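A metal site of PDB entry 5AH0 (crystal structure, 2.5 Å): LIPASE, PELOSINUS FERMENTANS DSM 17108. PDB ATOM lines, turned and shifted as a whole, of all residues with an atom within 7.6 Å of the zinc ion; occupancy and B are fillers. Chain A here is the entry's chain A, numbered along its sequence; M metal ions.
Of the 20 residues printed, 4 come within 4 Å of the zinc ion.
The nearest printed residue that does not touch the zinc ion is Trp 55 (4.4 Å).
The zinc ion is bound by OD1 of Asp 56 (1.9 Å), OD2 of Asp 233 (2.0 Å), NE2 of His 82 (2.1 Å) and NE2 of His 76 (2.1 Å).
The side-chain carboxylate of Asp 56 lies within hydrogen-bond range of the side-chain amide nitrogen of Gln 204, at 3.0 Å.
The side-chain carboxylate (OD1) of Asp 233 lies close to the side-chain hydroxyl (OG) of Ser 53 (3.3 Å).
The backbone NH (N) of Asp 233 is in hydrogen-bond range of the side-chain hydroxyl (OG1) of Thr 231, at 2.9 Å.
The backbone NH of His 82 is in hydrogen-bond range of the backbone carbonyl oxygen of Ser 77 (2.7 Å).
NE1 of Trp 55 sits close to ND1 of His 76, 3.5 Å away.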
ATOM      1  N   SER A  52       3.776   6.960 -19.511  1.00  0.00           N
ATOM      2  CA  SER A  52       2.754   6.017 -19.937  1.00  0.00           C
ATOM      3  C   SER A  52       1.420   6.713 -20.215  1.00  0.00           C
ATOM      4  O   SER A  52       1.244   7.907 -19.952  1.00  0.00           O
ATOM      5  CB  SER A  52       2.548   4.927 -18.881  1.00  0.00           C
ATOM      6  OG  SER A  52       3.755   4.232 -18.595  1.00  0.00           O
ATOM      7  N   SER A  53       0.476   5.928 -20.736  1.00  0.00           N
ATOM      8  CA  SER A  53      -0.911   6.349 -20.949  1.00  0.00           C
ATOM      9  C   SER A  53      -1.639   6.566 -19.614  1.00  0.00           C
ATOM     10  O   SER A  53      -1.218   6.059 -18.575  1.00  0.00           O
ATOM     11  CB  SER A  53      -1.644   5.297 -21.792  1.00  0.00           C
ATOM     12  OG  SER A  53      -3.055   5.445 -21.733  1.00  0.00           O
ATOM     13  N   ASN A  54      -2.757   7.289 -19.642  1.00  0.00           N
ATOM     14  CA  ASN A  54      -3.578   7.465 -18.463  1.00  0.00           C
ATOM     15  C   ASN A  54      -4.185   6.139 -18.014  1.00  0.00           C
ATOM     16  O   ASN A  54      -4.262   5.859 -16.818  1.00  0.00           O
ATOM     17  CB  ASN A  54      -4.665   8.507 -18.734  1.00  0.00           C
ATOM     18  CG  ASN A  54      -4.149   9.945 -18.609  1.00  0.00           C
ATOM     19  OD1 ASN A  54      -3.474  10.298 -17.631  1.00  0.00           O
ATOM     20  ND2 ASN A  54      -4.455  10.781 -19.595  1.00  0.00           N
ATOM     21  N   TRP A  55      -4.602   5.320 -18.971  1.00  0.00           N
ATOM     22  CA  TRP A  55      -5.093   3.980 -18.681  1.00  0.00           C
ATOM     23  C   TRP A  55      -4.040   3.193 -17.927  1.00  0.00           C
ATOM     24  O   TRP A  55      -4.332   2.561 -16.908  1.00  0.00           O
ATOM     25  CB  TRP A  55      -5.475   3.253 -19.972  1.00  0.00           C
ATOM     26  CG  TRP A  55      -5.997   1.845 -19.761  1.00  0.00           C
ATOM     27  CD1 TRP A  55      -5.252   0.717 -19.551  1.00  0.00           C
ATOM     28  CD2 TRP A  55      -7.364   1.419 -19.755  1.00  0.00           C
ATOM     29  NE1 TRP A  55      -6.066  -0.376 -19.409  1.00  0.00           N
ATOM     30  CE2 TRP A  55      -7.377   0.023 -19.542  1.00  0.00           C
ATOM     31  CE3 TRP A  55      -8.589   2.081 -19.924  1.00  0.00           C
ATOM     32  CZ2 TRP A  55      -8.554  -0.721 -19.483  1.00  0.00           C
ATOM     33  CZ3 TRP A  55      -9.761   1.346 -19.864  1.00  0.00           C
ATOM     34  CH2 TRP A  55      -9.731  -0.051 -19.639  1.00  0.00           C
ATOM     35  N   ASP A  56      -2.819   3.183 -18.446  1.00  0.00           N
ATOM     36  CA  ASP A  56      -1.725   2.480 -17.785  1.00  0.00           C
ATOM     37  C   ASP A  56      -1.436   3.061 -16.412  1.00  0.00           C
ATOM     38  O   ASP A  56      -1.249   2.319 -15.445  1.00  0.00           O
ATOM     39  CB  ASP A  56      -0.465   2.527 -18.641  1.00  0.00           C
ATOM     40  CG  ASP A  56      -0.512   1.550 -19.792  1.00  0.00           C
ATOM     41  OD1 ASP A  56      -1.621   1.200 -20.248  1.00  0.00           O
ATOM     42  OD2 ASP A  56       0.577   1.118 -20.234  1.00  0.00           O
ATOM     43  N   ARG A  57      -1.384   4.385 -16.321  1.00  0.00           N
ATOM     44  CA  ARG A  57      -1.083   5.034 -15.061  1.00  0.00           C
ATOM     45  C   ARG A  57      -2.198   4.777 -14.047  1.00  0.00           C
ATOM     46  O   ARG A  57      -1.935   4.577 -12.855  1.00  0.00           O
ATOM     47  CB  ARG A  57      -0.869   6.536 -15.259  1.00  0.00           C
ATOM     48  CG  ARG A  57       0.482   6.904 -15.851  1.00  0.00           C
ATOM     49  CD  ARG A  57       0.408   8.194 -16.644  1.00  0.00           C
ATOM     50  NE  ARG A  57      -0.016   9.327 -15.819  1.00  0.00           N
ATOM     51  CZ  ARG A  57       0.798  10.075 -15.087  1.00  0.00           C
ATOM     52  NH1 ARG A  57       2.101   9.812 -15.074  1.00  0.00           N
ATOM     53  NH2 ARG A  57       0.308  11.084 -14.368  1.00  0.00           N
ATOM     54  N   CYS A  59      -4.097   2.141 -13.863  1.00  0.00           N
ATOM     55  CA  CYS A  59      -3.927   0.760 -13.380  1.00  0.00           C
ATOM     56  C   CYS A  59      -2.768   0.666 -12.383  1.00  0.00           C
ATOM     57  O   CYS A  59      -2.865  -0.033 -11.372  1.00  0.00           O
ATOM     58  CB  CYS A  59      -3.698  -0.211 -14.529  1.00  0.00           C
ATOM     59  SG  CYS A  59      -5.102  -0.385 -15.626  1.00  0.00           S
ATOM     60  N   TYR A  72      -2.805  -4.249 -16.427  1.00  0.00           N
ATOM     61  CA  TYR A  72      -3.253  -3.304 -17.448  1.00  0.00           C
ATOM     62  C   TYR A  72      -4.525  -3.814 -18.135  1.00  0.00           C
ATOM     63  O   TYR A  72      -5.214  -3.046 -18.816  1.00  0.00           O
ATOM     64  CB  TYR A  72      -2.146  -3.065 -18.466  1.00  0.00           C
ATOM     65  CG  TYR A  72      -0.910  -2.475 -17.850  1.00  0.00           C
ATOM     66  CD1 TYR A  72      -0.896  -1.163 -17.375  1.00  0.00           C
ATOM     67  CD2 TYR A  72       0.247  -3.234 -17.711  1.00  0.00           C
ATOM     68  CE1 TYR A  72       0.242  -0.620 -16.792  1.00  0.00           C
ATOM     69  CE2 TYR A  72       1.390  -2.705 -17.129  1.00  0.00           C
ATOM     70  CZ  TYR A  72       1.372  -1.395 -16.673  1.00  0.00           C
ATOM     71  OH  TYR A  72       2.501  -0.871 -16.094  1.00  0.00           O
ATOM     72  N   HIS A  76      -7.140  -4.764 -23.079  1.00  0.00           N
ATOM     73  CA  HIS A  76      -6.317  -3.595 -23.355  1.00  0.00           C
ATOM     74  C   HIS A  76      -4.888  -3.972 -23.751  1.00  0.00           C
ATOM     75  O   HIS A  76      -4.385  -3.485 -24.764  1.00  0.00           O
ATOM     76  CB  HIS A  76      -6.264  -2.656 -22.155  1.00  0.00           C
ATOM     77  CG  HIS A  76      -5.318  -1.500 -22.337  1.00  0.00           C
ATOM     78  ND1 HIS A  76      -5.708  -0.298 -22.871  1.00  0.00           N
ATOM     79  CD2 HIS A  76      -3.996  -1.391 -22.084  1.00  0.00           C
ATOM     80  CE1 HIS A  76      -4.667   0.512 -22.937  1.00  0.00           C
ATOM     81  NE2 HIS A  76      -3.620  -0.133 -22.468  1.00  0.00           N
ATOM     82  N   SER A  77      -4.255  -4.823 -22.950  1.00  0.00           N
ATOM     83  CA  SER A  77      -2.871  -5.222 -23.174  1.00  0.00           C
ATOM     84  C   SER A  77      -2.666  -5.766 -24.576  1.00  0.00           C
ATOM     85  O   SER A  77      -1.763  -5.339 -25.291  1.00  0.00           O
ATOM     86  CB  SER A  77      -2.438  -6.292 -22.173  1.00  0.00           C
ATOM     87  OG  SER A  77      -2.896  -6.011 -20.872  1.00  0.00           O
ATOM     88  N   LYS A  80      -3.149  -3.288 -27.505  1.00  0.00           N
ATOM     89  CA  LYS A  80      -2.071  -2.321 -27.635  1.00  0.00           C
ATOM     90  C   LYS A  80      -0.709  -3.005 -27.807  1.00  0.00           C
ATOM     91  O   LYS A  80       0.245  -2.390 -28.286  1.00  0.00           O
ATOM     92  CB  LYS A  80      -2.044  -1.406 -26.425  1.00  0.00           C
ATOM     93  CG  LYS A  80      -2.779  -0.102 -26.631  1.00  0.00           C
ATOM     94  CD  LYS A  80      -4.281  -0.301 -26.735  1.00  0.00           C
ATOM     95  CE  LYS A  80      -5.025   1.009 -26.995  1.00  0.00           C
ATOM     96  NZ  LYS A  80      -5.132   1.317 -28.455  1.00  0.00           N
ATOM     97  N   GLY A  81      -0.609  -4.272 -27.422  1.00  0.00           N
ATOM     98  CA  GLY A  81       0.658  -4.977 -27.518  1.00  0.00           C
ATOM     99  C   GLY A  81       1.534  -4.818 -26.282  1.00  0.00           C
ATOM    100  O   GLY A  81       2.703  -4.457 -26.381  1.00  0.00           O
ATOM    101  N   HIS A  82       0.952  -5.113 -25.120  1.00  0.00           N
ATOM    102  CA  HIS A  82       1.621  -4.976 -23.817  1.00  0.00           C
ATOM    103  C   HIS A  82       2.296  -6.229 -23.297  1.00  0.00           C
ATOM    104  O   HIS A  82       2.375  -7.240 -23.969  1.00  0.00           O
ATOM    105  CB  HIS A  82       0.612  -4.562 -22.740  1.00  0.00           C
ATOM    106  CG  HIS A  82       0.387  -3.095 -22.611  1.00  0.00           C
ATOM    107  ND1 HIS A  82       1.255  -2.156 -23.134  1.00  0.00           N
ATOM    108  CD2 HIS A  82      -0.616  -2.400 -22.029  1.00  0.00           C
ATOM    109  CE1 HIS A  82       0.798  -0.947 -22.861  1.00  0.00           C
ATOM    110  NE2 HIS A  82      -0.337  -1.070 -22.200  1.00  0.00           N
ATOM    111  N   SER A  83       2.795  -6.095 -22.071  1.00  0.00           N
ATOM    112  CA  SER A  83       2.798  -7.170 -21.103  1.00  0.00           C
ATOM    113  C   SER A  83       1.549  -6.881 -20.295  1.00  0.00           C
ATOM    114  O   SER A  83       1.342  -5.740 -19.901  1.00  0.00           O
ATOM    115  CB  SER A  83       4.043  -7.163 -20.216  1.00  0.00           C
ATOM    116  OG  SER A  83       5.227  -7.094 -20.975  1.00  0.00           O
ATOM    117  N   GLN A 204       6.583  -2.753 -19.688  1.00  0.00           N
ATOM    118  CA  GLN A 204       5.506  -3.396 -20.434  1.00  0.00           C
ATOM    119  C   GLN A 204       5.690  -3.180 -21.933  1.00  0.00           C
ATOM    120  O   GLN A 204       4.897  -3.655 -22.749  1.00  0.00           O
ATOM    121  CB  GLN A 204       4.140  -2.880 -19.993  1.00  0.00           C
ATOM    122  CG  GLN A 204       3.756  -1.511 -20.524  1.00  0.00           C
ATOM    123  CD  GLN A 204       4.263  -0.373 -19.647  1.00  0.00           C
ATOM    124  OE1 GLN A 204       5.358  -0.444 -19.071  1.00  0.00           O
ATOM    125  NE2 GLN A 204       3.457   0.677 -19.530  1.00  0.00           N
ATOM    126  N   TRP A 205       6.755  -2.456 -22.284  1.00  0.00           N
ATOM    127  CA  TRP A 205       7.173  -2.299 -23.675  1.00  0.00           C
ATOM    128  C   TRP A 205       8.570  -2.850 -23.904  1.00  0.00           C
ATOM    129  O   TRP A 205       9.137  -2.682 -24.983  1.00  0.00           O
ATOM    130  CB  TRP A 205       7.143  -0.842 -24.090  1.00  0.00           C
ATOM    131  CG  TRP A 205       5.838  -0.131 -23.900  1.00  0.00           C
ATOM    132  CD1 TRP A 205       5.473   0.655 -22.842  1.00  0.00           C
ATOM    133  CD2 TRP A 205       4.720  -0.139 -24.795  1.00  0.00           C
ATOM    134  NE1 TRP A 205       4.195   1.142 -23.028  1.00  0.00           N
ATOM    135  CE2 TRP A 205       3.715   0.661 -24.220  1.00  0.00           C
ATOM    136  CE3 TRP A 205       4.469  -0.749 -26.036  1.00  0.00           C
ATOM    137  CZ2 TRP A 205       2.475   0.878 -24.837  1.00  0.00           C
ATOM    138  CZ3 TRP A 205       3.235  -0.538 -26.641  1.00  0.00           C
ATOM    139  CH2 TRP A 205       2.263   0.266 -26.047  1.00  0.00           C
ATOM    140  N   THR A 231       1.815   3.549 -31.627  1.00  0.00           N
ATOM    141  CA  THR A 231       0.716   3.354 -30.706  1.00  0.00           C
ATOM    142  C   THR A 231       0.058   4.668 -30.295  1.00  0.00           C
ATOM    143  O   THR A 231       0.610   5.742 -30.499  1.00  0.00           O
ATOM    144  CB  THR A 231       1.166   2.617 -29.439  1.00  0.00           C
ATOM    145  OG1 THR A 231       0.036   2.428 -28.576  1.00  0.00           O
ATOM    146  CG2 THR A 231       2.193   3.422 -28.705  1.00  0.00           C
ATOM    147  N   ASN A 232      -1.148   4.569 -29.734  1.00  0.00           N
ATOM    148  CA  ASN A 232      -1.807   5.728 -29.155  1.00  0.00           C
ATOM    149  C   ASN A 232      -1.933   5.540 -27.649  1.00  0.00           C
ATOM    150  O   ASN A 232      -2.799   6.124 -27.012  1.00  0.00           O
ATOM    151  CB  ASN A 232      -3.182   5.966 -29.785  1.00  0.00           C
ATOM    152  CG  ASN A 232      -4.170   4.851 -29.463  1.00  0.00           C
ATOM    153  OD1 ASN A 232      -3.775   3.719 -29.170  1.00  0.00           O
ATOM    154  ND2 ASN A 232      -5.451   5.167 -29.505  1.00  0.00           N
ATOM    155  N   ASP A 233      -1.066   4.688 -27.099  1.00  0.00           N
ATOM    156  CA  ASP A 233      -1.134   4.284 -25.698  1.00  0.00           C
ATOM    157  C   ASP A 233       0.005   4.833 -24.874  1.00  0.00           C
ATOM    158  O   ASP A 233       0.469   4.195 -23.934  1.00  0.00           O
ATOM    159  CB  ASP A 233      -1.160   2.752 -25.600  1.00  0.00           C
ATOM    160  CG  ASP A 233      -1.570   2.254 -24.219  1.00  0.00           C
ATOM    161  OD1 ASP A 233      -2.514   2.820 -23.638  1.00  0.00           O
ATOM    162  OD2 ASP A 233      -0.935   1.287 -23.726  1.00  0.00           O
ATOM    163  N   LEU A 234       0.468   6.030 -25.221  1.00  0.00           N
ATOM    164  CA  LEU A 234       1.494   6.684 -24.424  1.00  0.00           C
ATOM    165  C   LEU A 234       1.075   8.121 -24.090  1.00  0.00           C
ATOM    166  O   LEU A 234       0.062   8.614 -24.611  1.00  0.00           O
ATOM    167  CB  LEU A 234       2.821   6.659 -25.167  1.00  0.00           C
ATOM    168  CG  LEU A 234       3.447   5.260 -25.232  1.00  0.00           C
ATOM    169  CD1 LEU A 234       4.536   5.210 -26.283  1.00  0.00           C
ATOM    170  CD2 LEU A 234       3.991   4.867 -23.885  1.00  0.00           C
HETATM  171 ZN    ZN M   1      -1.677   0.506 -22.053  1.00  0.00          ZN
